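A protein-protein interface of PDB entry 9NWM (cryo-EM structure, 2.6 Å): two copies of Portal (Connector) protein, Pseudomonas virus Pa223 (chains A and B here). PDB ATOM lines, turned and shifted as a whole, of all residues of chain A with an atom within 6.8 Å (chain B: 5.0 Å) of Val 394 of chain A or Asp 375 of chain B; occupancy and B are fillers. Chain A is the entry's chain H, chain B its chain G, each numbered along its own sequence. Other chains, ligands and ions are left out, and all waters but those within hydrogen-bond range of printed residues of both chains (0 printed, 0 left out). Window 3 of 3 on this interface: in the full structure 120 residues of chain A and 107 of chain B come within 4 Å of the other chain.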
ATOM      1  N   GLN A 377     -33.585  24.201  -7.734  1.00  0.00           N
ATOM      2  CA  GLN A 377     -32.212  24.638  -7.537  1.00  0.00           C
ATOM      3  C   GLN A 377     -31.566  25.188  -8.797  1.00  0.00           C
ATOM      4  O   GLN A 377     -30.450  25.708  -8.718  1.00  0.00           O
ATOM      5  CB  GLN A 377     -31.358  23.480  -7.006  1.00  0.00           C
ATOM      6  CG  GLN A 377     -31.996  22.711  -5.873  1.00  0.00           C
ATOM      7  CD  GLN A 377     -31.858  23.420  -4.547  1.00  0.00           C
ATOM      8  OE1 GLN A 377     -30.822  23.336  -3.892  1.00  0.00           O
ATOM      9  NE2 GLN A 377     -32.903  24.127  -4.143  1.00  0.00           N
ATOM     10  N   VAL A 378     -32.232  25.102  -9.943  1.00  0.00           N
ATOM     11  CA  VAL A 378     -31.649  25.453 -11.231  1.00  0.00           C
ATOM     12  C   VAL A 378     -32.510  26.523 -11.881  1.00  0.00           C
ATOM     13  O   VAL A 378     -33.741  26.414 -11.889  1.00  0.00           O
ATOM     14  CB  VAL A 378     -31.528  24.221 -12.143  1.00  0.00           C
ATOM     15  CG1 VAL A 378     -31.066  24.627 -13.527  1.00  0.00           C
ATOM     16  CG2 VAL A 378     -30.579  23.210 -11.535  1.00  0.00           C
ATOM     17  N   ASN A 379     -31.865  27.551 -12.424  1.00  0.00           N
ATOM     18  CA  ASN A 379     -32.561  28.589 -13.177  1.00  0.00           C
ATOM     19  C   ASN A 379     -33.031  27.992 -14.495  1.00  0.00           C
ATOM     20  O   ASN A 379     -32.258  27.863 -15.444  1.00  0.00           O
ATOM     21  CB  ASN A 379     -31.641  29.781 -13.411  1.00  0.00           C
ATOM     22  CG  ASN A 379     -32.396  31.027 -13.808  1.00  0.00           C
ATOM     23  OD1 ASN A 379     -32.699  31.234 -14.979  1.00  0.00           O
ATOM     24  ND2 ASN A 379     -32.696  31.872 -12.832  1.00  0.00           N
ATOM     25  N   VAL A 392     -25.440  29.477 -16.847  1.00  0.00           N
ATOM     26  CA  VAL A 392     -26.580  28.905 -16.144  1.00  0.00           C
ATOM     27  C   VAL A 392     -26.336  29.065 -14.652  1.00  0.00           C
ATOM     28  O   VAL A 392     -25.331  28.572 -14.125  1.00  0.00           O
ATOM     29  CB  VAL A 392     -26.792  27.430 -16.513  1.00  0.00           C
ATOM     30  CG1 VAL A 392     -28.010  26.880 -15.804  1.00  0.00           C
ATOM     31  CG2 VAL A 392     -26.930  27.278 -18.011  1.00  0.00           C
ATOM     32  N   ARG A 393     -27.250  29.748 -13.971  1.00  0.00           N
ATOM     33  CA  ARG A 393     -27.108  30.021 -12.548  1.00  0.00           C
ATOM     34  C   ARG A 393     -27.790  28.929 -11.739  1.00  0.00           C
ATOM     35  O   ARG A 393     -28.946  28.583 -11.996  1.00  0.00           O
ATOM     36  CB  ARG A 393     -27.698  31.386 -12.201  1.00  0.00           C
ATOM     37  CG  ARG A 393     -26.815  32.551 -12.596  1.00  0.00           C
ATOM     38  CD  ARG A 393     -27.574  33.857 -12.524  1.00  0.00           C
ATOM     39  NE  ARG A 393     -28.569  33.962 -13.583  1.00  0.00           N
ATOM     40  CZ  ARG A 393     -28.977  35.104 -14.115  1.00  0.00           C
ATOM     41  NH1 ARG A 393     -28.505  36.267 -13.699  1.00  0.00           N
ATOM     42  NH2 ARG A 393     -29.882  35.078 -15.088  1.00  0.00           N
ATOM     43  N   VAL A 394     -27.069  28.385 -10.762  1.00  0.00           N
ATOM     44  CA  VAL A 394     -27.553  27.289  -9.935  1.00  0.00           C
ATOM     45  C   VAL A 394     -27.318  27.639  -8.473  1.00  0.00           C
ATOM     46  O   VAL A 394     -26.382  28.368  -8.134  1.00  0.00           O
ATOM     47  CB  VAL A 394     -26.861  25.956 -10.296  1.00  0.00           C
ATOM     48  CG1 VAL A 394     -27.582  24.800  -9.665  1.00  0.00           C
ATOM     49  CG2 VAL A 394     -26.816  25.769 -11.796  1.00  0.00           C
ATOM     50  N   LYS A 395     -28.183  27.118  -7.602  1.00  0.00           N
ATOM     51  CA  LYS A 395     -28.043  27.340  -6.170  1.00  0.00           C
ATOM     52  C   LYS A 395     -27.226  26.263  -5.471  1.00  0.00           C
ATOM     53  O   LYS A 395     -26.798  26.474  -4.332  1.00  0.00           O
ATOM     54  CB  LYS A 395     -29.419  27.433  -5.508  1.00  0.00           C
ATOM     55  CG  LYS A 395     -30.082  28.790  -5.654  1.00  0.00           C
ATOM     56  CD  LYS A 395     -31.582  28.701  -5.425  1.00  0.00           C
ATOM     57  CE  LYS A 395     -32.211  30.082  -5.302  1.00  0.00           C
ATOM     58  NZ  LYS A 395     -33.226  30.151  -4.213  1.00  0.00           N
ATOM     59  N   ALA A 396     -27.002  25.121  -6.118  1.00  0.00           N
ATOM     60  CA  ALA A 396     -26.211  24.048  -5.534  1.00  0.00           C
ATOM     61  C   ALA A 396     -25.809  23.089  -6.642  1.00  0.00           C
ATOM     62  O   ALA A 396     -26.623  22.767  -7.508  1.00  0.00           O
ATOM     63  CB  ALA A 396     -26.988  23.307  -4.440  1.00  0.00           C
ATOM     64  N   MET A 397     -24.563  22.632  -6.606  1.00  0.00           N
ATOM     65  CA  MET A 397     -24.066  21.778  -7.671  1.00  0.00           C
ATOM     66  C   MET A 397     -24.595  20.354  -7.563  1.00  0.00           C
ATOM     67  O   MET A 397     -25.445  20.029  -6.730  1.00  0.00           O
ATOM     68  CB  MET A 397     -22.547  21.760  -7.700  1.00  0.00           C
ATOM     69  CG  MET A 397     -21.904  23.089  -7.907  1.00  0.00           C
ATOM     70  SD  MET A 397     -21.937  23.258  -9.692  1.00  0.00           S
ATOM     71  CE  MET A 397     -20.937  21.844 -10.127  1.00  0.00           C
ATOM     72  N   ASN A 398     -24.058  19.493  -8.430  1.00  0.00           N
ATOM     73  CA  ASN A 398     -24.562  18.140  -8.634  1.00  0.00           C
ATOM     74  C   ASN A 398     -26.059  18.172  -8.920  1.00  0.00           C
ATOM     75  O   ASN A 398     -26.844  17.396  -8.373  1.00  0.00           O
ATOM     76  CB  ASN A 398     -24.240  17.244  -7.438  1.00  0.00           C
ATOM     77  CG  ASN A 398     -22.752  17.049  -7.246  1.00  0.00           C
ATOM     78  OD1 ASN A 398     -22.061  16.549  -8.132  1.00  0.00           O
ATOM     79  ND2 ASN A 398     -22.247  17.449  -6.085  1.00  0.00           N
ATOM     80  N   SER A 399     -26.452  19.099  -9.794  1.00  0.00           N
ATOM     81  CA  SER A 399     -27.856  19.356 -10.060  1.00  0.00           C
ATOM     82  C   SER A 399     -28.265  19.194 -11.515  1.00  0.00           C
ATOM     83  O   SER A 399     -29.450  18.971 -11.773  1.00  0.00           O
ATOM     84  CB  SER A 399     -28.228  20.775  -9.609  1.00  0.00           C
ATOM     85  OG  SER A 399     -27.532  21.733 -10.379  1.00  0.00           O
ATOM     86  N   ILE A 400     -27.342  19.304 -12.465  1.00  0.00           N
ATOM     87  CA  ILE A 400     -27.648  19.137 -13.882  1.00  0.00           C
ATOM     88  C   ILE A 400     -26.666  18.139 -14.464  1.00  0.00           C
ATOM     89  O   ILE A 400     -25.451  18.357 -14.393  1.00  0.00           O
ATOM     90  CB  ILE A 400     -27.564  20.459 -14.659  1.00  0.00           C
ATOM     91  CG1 ILE A 400     -28.319  21.567 -13.936  1.00  0.00           C
ATOM     92  CG2 ILE A 400     -28.097  20.278 -16.066  1.00  0.00           C
ATOM     93  CD1 ILE A 400     -27.959  22.933 -14.433  1.00  0.00           C
ATOM     94  N   VAL B 372     -21.550  26.443 -15.829  1.00  0.00           N
ATOM     95  CA  VAL B 372     -22.419  26.446 -14.663  1.00  0.00           C
ATOM     96  C   VAL B 372     -21.714  27.204 -13.549  1.00  0.00           C
ATOM     97  O   VAL B 372     -20.522  26.974 -13.284  1.00  0.00           O
ATOM     98  CB  VAL B 372     -22.769  25.016 -14.224  1.00  0.00           C
ATOM     99  CG1 VAL B 372     -23.456  25.025 -12.878  1.00  0.00           C
ATOM    100  CG2 VAL B 372     -23.647  24.350 -15.261  1.00  0.00           C
ATOM    101  N   VAL B 373     -22.456  28.107 -12.905  1.00  0.00           N
ATOM    102  CA  VAL B 373     -21.944  29.034 -11.904  1.00  0.00           C
ATOM    103  C   VAL B 373     -22.879  29.020 -10.703  1.00  0.00           C
ATOM    104  O   VAL B 373     -24.103  29.071 -10.866  1.00  0.00           O
ATOM    105  CB  VAL B 373     -21.834  30.461 -12.474  1.00  0.00           C
ATOM    106  CG1 VAL B 373     -21.451  31.440 -11.392  1.00  0.00           C
ATOM    107  CG2 VAL B 373     -20.833  30.501 -13.608  1.00  0.00           C
ATOM    108  N   LEU B 374     -22.310  28.954  -9.499  1.00  0.00           N
ATOM    109  CA  LEU B 374     -23.106  29.097  -8.284  1.00  0.00           C
ATOM    110  C   LEU B 374     -23.613  30.526  -8.163  1.00  0.00           C
ATOM    111  O   LEU B 374     -22.835  31.479  -8.266  1.00  0.00           O
ATOM    112  CB  LEU B 374     -22.287  28.728  -7.051  1.00  0.00           C
ATOM    113  CG  LEU B 374     -22.165  27.255  -6.681  1.00  0.00           C
ATOM    114  CD1 LEU B 374     -21.201  27.092  -5.526  1.00  0.00           C
ATOM    115  CD2 LEU B 374     -23.526  26.705  -6.313  1.00  0.00           C
ATOM    116  N   ASP B 375     -24.912  30.677  -7.928  1.00  0.00           N
ATOM    117  CA  ASP B 375     -25.496  32.004  -7.810  1.00  0.00           C
ATOM    118  C   ASP B 375     -25.202  32.593  -6.437  1.00  0.00           C
ATOM    119  O   ASP B 375     -25.383  31.929  -5.413  1.00  0.00           O
ATOM    120  CB  ASP B 375     -27.002  31.941  -8.048  1.00  0.00           C
ATOM    121  CG  ASP B 375     -27.599  33.299  -8.337  1.00  0.00           C
ATOM    122  OD1 ASP B 375     -26.865  34.176  -8.840  1.00  0.00           O
ATOM    123  OD2 ASP B 375     -28.801  33.493  -8.065  1.00  0.00           O
ATOM    124  N   GLY B 376     -24.748  33.843  -6.419  1.00  0.00           N
ATOM    125  CA  GLY B 376     -24.465  34.539  -5.186  1.00  0.00           C
ATOM    126  C   GLY B 376     -23.083  34.310  -4.619  1.00  0.00           C
ATOM    127  O   GLY B 376     -22.733  34.939  -3.614  1.00  0.00           O
ATOM    128  N   GLN B 377     -22.285  33.436  -5.227  1.00  0.00           N
ATOM    129  CA  GLN B 377     -20.943  33.154  -4.746  1.00  0.00           C
ATOM    130  C   GLN B 377     -19.853  33.625  -5.694  1.00  0.00           C
ATOM    131  O   GLN B 377     -18.676  33.575  -5.326  1.00  0.00           O
ATOM    132  CB  GLN B 377     -20.772  31.648  -4.506  1.00  0.00           C
ATOM    133  CG  GLN B 377     -21.727  31.064  -3.486  1.00  0.00           C
ATOM    134  CD  GLN B 377     -21.535  31.648  -2.106  1.00  0.00           C
ATOM    135  OE1 GLN B 377     -20.544  31.370  -1.436  1.00  0.00           O
ATOM    136  NE2 GLN B 377     -22.486  32.463  -1.673  1.00  0.00           N
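1 position is printed for both chains. Of the 11 pairs that touch across the chains among the printed residues, none has its exchanged pair printed and touching as well.
Among the printed residues, merely in contact across the chains: Val 392 of chain A with Val 372 of chain B, Arg 393 of chain A with Val 373 of chain B, Arg 393 of chain A with Asp 375 of chain B, Val 394 of chain A with Val 372 of chain B, Val 394 of chain A with Leu 374 of chain B, Lys 395 of chain A with Leu 374 of chain B, Ala 396 of chain A with Leu 374 of chain B and Met 397 of chain A with Val 372 of chain B.
The backbone carbonyl oxygen (O) of Ala 396 of chain A lies within hydrogen-bond range of the side-chain hydroxyl (OG) of Ser 399 of chain A (3.2 Å). N of Asn 379 of chain A sits at hydrogen-bond distance from O of Arg 393 of chain A, at 3.1 Å. O of Gln 377 of chain A sits at hydrogen-bond distance from N of Lys 395 of chain A, 2.9 Å away.
Val 394 of chain A touches just these residues of chain B: Val 372 (3.6 Å), Val 373 (3.0 Å), Leu 374 (3.4 Å) and Asp 375 (2.7 Å). Asp 375 of chain B touches two residues of chain A. Of the printed residues of chain B, Arg 393 of chain A touches Val 373 (3.6 Å) and Asp 375 (3.8 Å). Of the printed residues of chain A, Val 373 of chain B touches Val 392, Arg 393 and Val 394. Printed residues of chain B within 4 Å of Ala 396 of chain A: Leu 374. Of the printed residues of chain B, Met 397 of chain A touches Val 372 (3.9 Å). Of the printed residues of chain B, Val 392 of chain A touches Val 372 and Val 373. Gly 376 of chain B touches none of the printed residues of chain A.
Hydrophobic or aromatic side chains of chain B that line the printed part of chain A: Val 372 and Leu 374. Along chain B the printed residues that touch a printed residue of chain A span positions 372 to 375. Of the 12 printed residues of chain A, 6 touch a printed residue of chain B. Hydrophobic or aromatic side chains of chain A that line the printed part of chain B: Val 394 and Met 397. Among the printed residues, 11 pairs touch across the chains. Among the printed residues, no Asp or Glu carboxylate lies within 4 Å of a Lys or Arg side-chain nitrogen of the other chain.
The backbone carbonyl oxygen of Val 392 of chain A is in hydrogen-bond range of the backbone NH of Val 373 of chain B (3.2 Å). The backbone NH of Asp 375 of chain B is in hydrogen-bond range of the backbone carbonyl oxygen of Val 394 of chain A (2.7 Å). O of Val 373 of chain B lies within hydrogen-bond range of N of Val 394 of chain A, at 3.0 Å.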
